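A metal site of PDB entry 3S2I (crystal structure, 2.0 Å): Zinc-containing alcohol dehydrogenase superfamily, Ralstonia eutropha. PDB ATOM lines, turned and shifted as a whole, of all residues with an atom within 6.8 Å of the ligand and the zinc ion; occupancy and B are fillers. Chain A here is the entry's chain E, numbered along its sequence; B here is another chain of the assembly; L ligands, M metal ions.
A ring nitrogen (ND1) of His 63 lies close to the side-chain carboxylate of Asp 43, 3.4 Å away. The side-chain carboxylate of Glu 64 lies close to the backbone NH of Cys 150, 3.4 Å away. The backbone carbonyl oxygen (O) of Cys 150 lies within hydrogen-bond range of the side-chain hydroxyl (OG1) of Thr 154 (2.7 Å). The backbone NH (N) of Thr 42 sits close to the side-chain sulfur (SG) of Cys 40 (3.4 Å). The side-chain sulfur (SG) of Cys 40 lies close to the guanidinium group (NH1) of Arg 333, 3.6 Å away. N of Cys 40 sits at hydrogen-bond distance from OD2 of Asp 43, 2.8 Å away. The indole nitrogen (NE1) of Trp 89 lies close to the side-chain amide nitrogen (ND2) of Asn 113.
The side-chain hydroxyl (OG1) of Thr 42 is in hydrogen-bond range of an oxygen (O1) of the ligand (3.1 Å).
Residues that only touch the ligand: Ile 287, Trp 89, Trp 51, Leu 264, Val 288 and Leu 278 of chain B. Hydrophobic or aromatic side chains within 4 Å of the ligand: Trp 51, His 63, Trp 89, Leu 264, Ile 287, Val 288 and Leu 278 of chain B. Ten residues have an atom within 4 Å of the ligand: Cys 40, Thr 42, Trp 51, His 63, Trp 89, Cys 150, Leu 264, Ile 287, Val 288 and Leu 278 of chain B. The nearest printed residue that does not touch the ligand is Thr 154 (5.6 Å).
The zinc ion is bound by an oxygen (O2) of the ligand (2.1 Å), a ring nitrogen (NE2) of His 63 (2.2 Å), the side-chain sulfur of Cys 150 (2.3 Å) and the side-chain sulfur of Cys 40 (2.5 Å).
The nearest printed residue that does not touch the zinc ion is Thr 42 (4.01 Å).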
ATOM      1  N   VAL A  39      -4.874  10.485  18.165  1.00  0.00           N
ATOM      2  CA  VAL A  39      -4.172  10.714  16.898  1.00  0.00           C
ATOM      3  C   VAL A  39      -4.866  10.021  15.735  1.00  0.00           C
ATOM      4  O   VAL A  39      -5.100   8.812  15.762  1.00  0.00           O
ATOM      5  CB  VAL A  39      -2.698  10.255  16.979  1.00  0.00           C
ATOM      6  CG1 VAL A  39      -2.125  10.105  15.584  1.00  0.00           C
ATOM      7  CG2 VAL A  39      -1.886  11.230  17.807  1.00  0.00           C
ATOM      8  N   CYS A  40      -5.210  10.805  14.718  1.00  0.00           N
ATOM      9  CA  CYS A  40      -5.893  10.285  13.545  1.00  0.00           C
ATOM     10  C   CYS A  40      -4.982  10.351  12.324  1.00  0.00           C
ATOM     11  O   CYS A  40      -4.044  11.151  12.289  1.00  0.00           O
ATOM     12  CB  CYS A  40      -7.171  11.091  13.278  1.00  0.00           C
ATOM     13  SG  CYS A  40      -8.059  10.564  11.811  1.00  0.00           S
ATOM     14  N   HIS A  41      -5.238   9.499  11.347  1.00  0.00           N
ATOM     15  CA  HIS A  41      -4.451   9.509  10.121  1.00  0.00           C
ATOM     16  C   HIS A  41      -4.523  10.869   9.444  1.00  0.00           C
ATOM     17  O   HIS A  41      -3.579  11.309   8.782  1.00  0.00           O
ATOM     18  CB  HIS A  41      -4.933   8.409   9.166  1.00  0.00           C
ATOM     19  CG  HIS A  41      -3.951   7.297   8.988  1.00  0.00           C
ATOM     20  ND1 HIS A  41      -2.996   7.304   7.990  1.00  0.00           N
ATOM     21  CD2 HIS A  41      -3.763   6.155   9.688  1.00  0.00           C
ATOM     22  CE1 HIS A  41      -2.271   6.201   8.081  1.00  0.00           C
ATOM     23  NE2 HIS A  41      -2.717   5.487   9.101  1.00  0.00           N
ATOM     24  N   THR A  42      -5.657  11.546   9.613  1.00  0.00           N
ATOM     25  CA  THR A  42      -5.860  12.880   9.066  1.00  0.00           C
ATOM     26  C   THR A  42      -4.793  13.858   9.557  1.00  0.00           C
ATOM     27  O   THR A  42      -4.424  14.787   8.843  1.00  0.00           O
ATOM     28  CB  THR A  42      -7.264  13.407   9.428  1.00  0.00           C
ATOM     29  OG1 THR A  42      -8.247  12.716   8.639  1.00  0.00           O
ATOM     30  CG2 THR A  42      -7.370  14.894   9.169  1.00  0.00           C
ATOM     31  N   ASP A  43      -4.307  13.644  10.777  1.00  0.00           N
ATOM     32  CA  ASP A  43      -3.260  14.485  11.332  1.00  0.00           C
ATOM     33  C   ASP A  43      -2.000  14.425  10.477  1.00  0.00           C
ATOM     34  O   ASP A  43      -1.311  15.425  10.292  1.00  0.00           O
ATOM     35  CB  ASP A  43      -2.949  14.085  12.771  1.00  0.00           C
ATOM     36  CG  ASP A  43      -4.136  14.264  13.704  1.00  0.00           C
ATOM     37  OD1 ASP A  43      -4.953  15.184  13.449  1.00  0.00           O
ATOM     38  OD2 ASP A  43      -4.269  13.493  14.674  1.00  0.00           O
ATOM     39  N   TRP A  51      -3.572  16.929   0.777  1.00  0.00           N
ATOM     40  CA  TRP A  51      -4.949  17.363   0.535  1.00  0.00           C
ATOM     41  C   TRP A  51      -5.028  18.666  -0.263  1.00  0.00           C
ATOM     42  O   TRP A  51      -4.225  19.575  -0.045  1.00  0.00           O
ATOM     43  CB  TRP A  51      -5.712  17.479   1.860  1.00  0.00           C
ATOM     44  CG  TRP A  51      -5.890  16.159   2.540  1.00  0.00           C
ATOM     45  CD1 TRP A  51      -5.361  14.958   2.168  1.00  0.00           C
ATOM     46  CD2 TRP A  51      -6.656  15.902   3.733  1.00  0.00           C
ATOM     47  NE1 TRP A  51      -5.746  13.979   3.038  1.00  0.00           N
ATOM     48  CE2 TRP A  51      -6.542  14.522   4.006  1.00  0.00           C
ATOM     49  CE3 TRP A  51      -7.428  16.701   4.582  1.00  0.00           C
ATOM     50  CZ2 TRP A  51      -7.171  13.930   5.100  1.00  0.00           C
ATOM     51  CZ3 TRP A  51      -8.057  16.112   5.659  1.00  0.00           C
ATOM     52  CH2 TRP A  51      -7.915  14.736   5.914  1.00  0.00           C
ATOM     53  N   HIS A  63      -7.904  16.769  16.479  1.00  0.00           N
ATOM     54  CA  HIS A  63      -9.364  16.914  16.505  1.00  0.00           C
ATOM     55  C   HIS A  63      -9.996  15.761  17.253  1.00  0.00           C
ATOM     56  O   HIS A  63     -11.157  15.422  17.031  1.00  0.00           O
ATOM     57  CB  HIS A  63      -9.902  16.971  15.078  1.00  0.00           C
ATOM     58  CG  HIS A  63      -9.418  15.866  14.208  1.00  0.00           C
ATOM     59  ND1 HIS A  63      -8.233  15.940  13.508  1.00  0.00           N
ATOM     60  CD2 HIS A  63      -9.926  14.636  13.947  1.00  0.00           C
ATOM     61  CE1 HIS A  63      -8.042  14.817  12.832  1.00  0.00           C
ATOM     62  NE2 HIS A  63      -9.059  14.006  13.090  1.00  0.00           N
ATOM     63  N   GLU A  64      -9.210  15.127  18.124  1.00  0.00           N
ATOM     64  CA  GLU A  64      -9.719  14.116  19.040  1.00  0.00           C
ATOM     65  C   GLU A  64      -9.291  14.478  20.458  1.00  0.00           C
ATOM     66  O   GLU A  64      -8.946  13.608  21.266  1.00  0.00           O
ATOM     67  CB  GLU A  64      -9.216  12.730  18.654  1.00  0.00           C
ATOM     68  CG  GLU A  64      -9.984  12.091  17.497  1.00  0.00           C
ATOM     69  CD  GLU A  64      -9.614  10.642  17.279  1.00  0.00           C
ATOM     70  OE1 GLU A  64      -8.524  10.224  17.738  1.00  0.00           O
ATOM     71  OE2 GLU A  64     -10.407   9.907  16.652  1.00  0.00           O
ATOM     72  N   TRP A  89     -13.457  17.093  14.816  1.00  0.00           N
ATOM     73  CA  TRP A  89     -13.164  17.645  13.497  1.00  0.00           C
ATOM     74  C   TRP A  89     -14.029  18.843  13.111  1.00  0.00           C
ATOM     75  O   TRP A  89     -13.510  19.868  12.673  1.00  0.00           O
ATOM     76  CB  TRP A  89     -13.287  16.545  12.443  1.00  0.00           C
ATOM     77  CG  TRP A  89     -13.105  17.024  11.032  1.00  0.00           C
ATOM     78  CD1 TRP A  89     -14.078  17.194  10.096  1.00  0.00           C
ATOM     79  CD2 TRP A  89     -11.873  17.415  10.410  1.00  0.00           C
ATOM     80  NE1 TRP A  89     -13.529  17.655   8.923  1.00  0.00           N
ATOM     81  CE2 TRP A  89     -12.180  17.802   9.087  1.00  0.00           C
ATOM     82  CE3 TRP A  89     -10.542  17.463  10.839  1.00  0.00           C
ATOM     83  CZ2 TRP A  89     -11.198  18.236   8.193  1.00  0.00           C
ATOM     84  CZ3 TRP A  89      -9.574  17.896   9.946  1.00  0.00           C
ATOM     85  CH2 TRP A  89      -9.908  18.279   8.640  1.00  0.00           C
ATOM     86  N   GLN A 111     -17.882  25.837   7.465  1.00  0.00           N
ATOM     87  CA  GLN A 111     -17.368  25.126   8.636  1.00  0.00           C
ATOM     88  C   GLN A 111     -15.890  25.392   8.894  1.00  0.00           C
ATOM     89  O   GLN A 111     -15.110  25.630   7.966  1.00  0.00           O
ATOM     90  CB  GLN A 111     -17.596  23.613   8.486  1.00  0.00           C
ATOM     91  CG  GLN A 111     -16.657  22.936   7.495  1.00  0.00           C
ATOM     92  CD  GLN A 111     -16.928  21.441   7.367  1.00  0.00           C
ATOM     93  OE1 GLN A 111     -16.209  20.617   7.936  1.00  0.00           O
ATOM     94  NE2 GLN A 111     -17.973  21.096   6.618  1.00  0.00           N
ATOM     95  N   ASN A 113     -12.537  23.554  10.880  1.00  0.00           N
ATOM     96  CA  ASN A 113     -12.139  22.217  11.274  1.00  0.00           C
ATOM     97  C   ASN A 113     -10.997  22.204  12.285  1.00  0.00           C
ATOM     98  O   ASN A 113      -9.961  22.839  12.071  1.00  0.00           O
ATOM     99  CB  ASN A 113     -11.786  21.389  10.048  1.00  0.00           C
ATOM    100  CG  ASN A 113     -12.972  21.211   9.110  1.00  0.00           C
ATOM    101  OD1 ASN A 113     -12.907  21.584   7.936  1.00  0.00           O
ATOM    102  ND2 ASN A 113     -14.055  20.664   9.634  1.00  0.00           N
ATOM    103  N   TYR A 116      -6.823  21.927  11.936  1.00  0.00           N
ATOM    104  CA  TYR A 116      -6.626  22.003  10.488  1.00  0.00           C
ATOM    105  C   TYR A 116      -6.769  23.428   9.984  1.00  0.00           C
ATOM    106  O   TYR A 116      -5.836  23.982   9.401  1.00  0.00           O
ATOM    107  CB  TYR A 116      -7.609  21.085   9.758  1.00  0.00           C
ATOM    108  CG  TYR A 116      -7.166  20.728   8.365  1.00  0.00           C
ATOM    109  CD1 TYR A 116      -6.590  19.497   8.086  1.00  0.00           C
ATOM    110  CD2 TYR A 116      -7.291  21.636   7.322  1.00  0.00           C
ATOM    111  CE1 TYR A 116      -6.175  19.168   6.805  1.00  0.00           C
ATOM    112  CE2 TYR A 116      -6.884  21.328   6.040  1.00  0.00           C
ATOM    113  CZ  TYR A 116      -6.321  20.090   5.795  1.00  0.00           C
ATOM    114  OH  TYR A 116      -5.914  19.773   4.516  1.00  0.00           O
ATOM    115  N   LEU A 149     -14.388  10.488  19.179  1.00  0.00           N
ATOM    116  CA  LEU A 149     -14.577  11.843  18.652  1.00  0.00           C
ATOM    117  C   LEU A 149     -14.352  11.915  17.144  1.00  0.00           C
ATOM    118  O   LEU A 149     -14.769  12.868  16.500  1.00  0.00           O
ATOM    119  CB  LEU A 149     -13.648  12.840  19.369  1.00  0.00           C
ATOM    120  CG  LEU A 149     -14.078  13.337  20.751  1.00  0.00           C
ATOM    121  CD1 LEU A 149     -15.449  13.989  20.688  1.00  0.00           C
ATOM    122  CD2 LEU A 149     -14.083  12.210  21.770  1.00  0.00           C
ATOM    123  N   CYS A 150     -13.690  10.907  16.597  1.00  0.00           N
ATOM    124  CA  CYS A 150     -13.506  10.852  15.155  1.00  0.00           C
ATOM    125  C   CYS A 150     -13.700   9.453  14.584  1.00  0.00           C
ATOM    126  O   CYS A 150     -14.605   9.237  13.782  1.00  0.00           O
ATOM    127  CB  CYS A 150     -12.144  11.391  14.737  1.00  0.00           C
ATOM    128  SG  CYS A 150     -12.008  11.537  12.952  1.00  0.00           S
ATOM    129  N   ALA A 151     -12.837   8.521  14.970  1.00  0.00           N
ATOM    130  CA  ALA A 151     -12.945   7.145  14.482  1.00  0.00           C
ATOM    131  C   ALA A 151     -14.338   6.580  14.755  1.00  0.00           C
ATOM    132  O   ALA A 151     -14.986   6.056  13.850  1.00  0.00           O
ATOM    133  CB  ALA A 151     -11.881   6.274  15.137  1.00  0.00           C
ATOM    134  N   THR A 154     -17.209   8.476  12.916  1.00  0.00           N
ATOM    135  CA  THR A 154     -17.023   8.268  11.476  1.00  0.00           C
ATOM    136  C   THR A 154     -17.593   6.916  11.013  1.00  0.00           C
ATOM    137  O   THR A 154     -18.334   6.861  10.036  1.00  0.00           O
ATOM    138  CB  THR A 154     -15.535   8.346  11.072  1.00  0.00           C
ATOM    139  OG1 THR A 154     -15.079   9.704  11.211  1.00  0.00           O
ATOM    140  CG2 THR A 154     -15.351   7.914   9.628  1.00  0.00           C
ATOM    141  N   LEU A 178     -10.052   2.956  12.632  1.00  0.00           N
ATOM    142  CA  LEU A 178     -11.480   3.050  12.378  1.00  0.00           C
ATOM    143  C   LEU A 178     -12.108   1.657  12.356  1.00  0.00           C
ATOM    144  O   LEU A 178     -13.017   1.367  13.120  1.00  0.00           O
ATOM    145  CB  LEU A 178     -11.749   3.757  11.046  1.00  0.00           C
ATOM    146  CG  LEU A 178     -12.047   5.258  11.106  1.00  0.00           C
ATOM    147  CD1 LEU A 178     -10.855   6.045  11.642  1.00  0.00           C
ATOM    148  CD2 LEU A 178     -12.461   5.758   9.730  1.00  0.00           C
ATOM    149  N   LEU A 264      -9.643   8.276   2.818  1.00  0.00           N
ATOM    150  CA  LEU A 264      -9.283   9.485   2.088  1.00  0.00           C
ATOM    151  C   LEU A 264      -7.945   9.356   1.359  1.00  0.00           C
ATOM    152  O   LEU A 264      -7.071  10.216   1.507  1.00  0.00           O
ATOM    153  CB  LEU A 264      -9.247  10.690   3.024  1.00  0.00           C
ATOM    154  CG  LEU A 264     -10.587  11.169   3.581  1.00  0.00           C
ATOM    155  CD1 LEU A 264     -10.399  12.413   4.436  1.00  0.00           C
ATOM    156  CD2 LEU A 264     -11.556  11.443   2.441  1.00  0.00           C
ATOM    157  N   ILE A 287     -18.834  11.614   5.683  1.00  0.00           N
ATOM    158  CA  ILE A 287     -17.915  12.531   6.374  1.00  0.00           C
ATOM    159  C   ILE A 287     -18.155  12.598   7.872  1.00  0.00           C
ATOM    160  O   ILE A 287     -19.136  13.198   8.328  1.00  0.00           O
ATOM    161  CB  ILE A 287     -18.004  13.966   5.788  1.00  0.00           C
ATOM    162  CG1 ILE A 287     -17.036  14.901   6.510  1.00  0.00           C
ATOM    163  CG2 ILE A 287     -19.422  14.500   5.859  1.00  0.00           C
ATOM    164  CD1 ILE A 287     -15.589  14.545   6.294  1.00  0.00           C
ATOM    165  N   VAL A 288     -17.259  11.980   8.643  1.00  0.00           N
ATOM    166  CA  VAL A 288     -17.387  11.947  10.102  1.00  0.00           C
ATOM    167  C   VAL A 288     -18.853  11.840  10.512  1.00  0.00           C
ATOM    168  O   VAL A 288     -19.537  10.899  10.114  1.00  0.00           O
ATOM    169  CB  VAL A 288     -16.698  13.154  10.782  1.00  0.00           C
ATOM    170  CG1 VAL A 288     -15.192  13.033  10.658  1.00  0.00           C
ATOM    171  CG2 VAL A 288     -17.171  14.475  10.176  1.00  0.00           C
ATOM    172  N   ARG A 333      -5.845   2.335  17.941  1.00  0.00           N
ATOM    173  CA  ARG A 333      -5.582   3.764  17.905  1.00  0.00           C
ATOM    174  C   ARG A 333      -4.465   4.176  18.858  1.00  0.00           C
ATOM    175  O   ARG A 333      -4.133   3.453  19.792  1.00  0.00           O
ATOM    176  CB  ARG A 333      -6.860   4.556  18.223  1.00  0.00           C
ATOM    177  CG  ARG A 333      -7.826   4.646  17.068  1.00  0.00           C
ATOM    178  CD  ARG A 333      -7.278   5.523  15.956  1.00  0.00           C
ATOM    179  NE  ARG A 333      -8.013   6.780  15.841  1.00  0.00           N
ATOM    180  CZ  ARG A 333      -8.252   7.409  14.693  1.00  0.00           C
ATOM    181  NH1 ARG A 333      -8.934   8.542  14.683  1.00  0.00           N
ATOM    182  NH2 ARG A 333      -7.814   6.885  13.559  1.00  0.00           N
ATOM    183  N   PHE B 274     -11.595  11.017  -2.662  1.00  0.00           N
ATOM    184  CA  PHE B 274     -11.451  12.165  -1.770  1.00  0.00           C
ATOM    185  C   PHE B 274     -12.660  13.086  -1.825  1.00  0.00           C
ATOM    186  O   PHE B 274     -13.303  13.332  -0.803  1.00  0.00           O
ATOM    187  CB  PHE B 274     -10.186  12.943  -2.112  1.00  0.00           C
ATOM    188  CG  PHE B 274      -9.765  13.921  -1.054  1.00  0.00           C
ATOM    189  CD1 PHE B 274      -8.864  13.548  -0.070  1.00  0.00           C
ATOM    190  CD2 PHE B 274     -10.285  15.205  -1.025  1.00  0.00           C
ATOM    191  CE1 PHE B 274      -8.476  14.434   0.914  1.00  0.00           C
ATOM    192  CE2 PHE B 274      -9.904  16.094  -0.034  1.00  0.00           C
ATOM    193  CZ  PHE B 274      -8.996  15.712   0.930  1.00  0.00           C
ATOM    194  N   VAL B 277     -16.025  11.568  -0.654  1.00  0.00           N
ATOM    195  CA  VAL B 277     -16.124  11.401   0.798  1.00  0.00           C
ATOM    196  C   VAL B 277     -16.334  12.734   1.524  1.00  0.00           C
ATOM    197  O   VAL B 277     -17.259  12.871   2.330  1.00  0.00           O
ATOM    198  CB  VAL B 277     -14.900  10.670   1.373  1.00  0.00           C
ATOM    199  CG1 VAL B 277     -14.977  10.625   2.893  1.00  0.00           C
ATOM    200  CG2 VAL B 277     -14.817   9.263   0.815  1.00  0.00           C
ATOM    201  N   LEU B 278     -15.468  13.706   1.252  1.00  0.00           N
ATOM    202  CA  LEU B 278     -15.594  15.019   1.878  1.00  0.00           C
ATOM    203  C   LEU B 278     -16.922  15.683   1.553  1.00  0.00           C
ATOM    204  O   LEU B 278     -17.484  16.401   2.385  1.00  0.00           O
ATOM    205  CB  LEU B 278     -14.438  15.939   1.453  1.00  0.00           C
ATOM    206  CG  LEU B 278     -13.245  16.008   2.394  1.00  0.00           C
ATOM    207  CD1 LEU B 278     -13.672  16.563   3.757  1.00  0.00           C
ATOM    208  CD2 LEU B 278     -12.590  14.651   2.542  1.00  0.00           C
HETATM  209  C1  LIG L   1     -11.224  13.560  10.165  1.00  0.00           C
HETATM  210  C2  LIG L   1     -11.556  14.145   8.843  1.00  0.00           C
HETATM  211  O1  LIG L   1     -10.704  14.331   7.816  1.00  0.00           O
HETATM  212  C3  LIG L   1     -11.326  14.878   6.760  1.00  0.00           C
HETATM  213  C4  LIG L   1     -12.653  15.053   7.116  1.00  0.00           C
HETATM  214  C5  LIG L   1     -12.803  14.591   8.417  1.00  0.00           C
HETATM  215  O2  LIG L   1     -10.126  12.738  10.212  1.00  0.00           O
HETATM  216 ZN    ZN M   1      -9.913  12.156  12.243  1.00  0.00          ZN
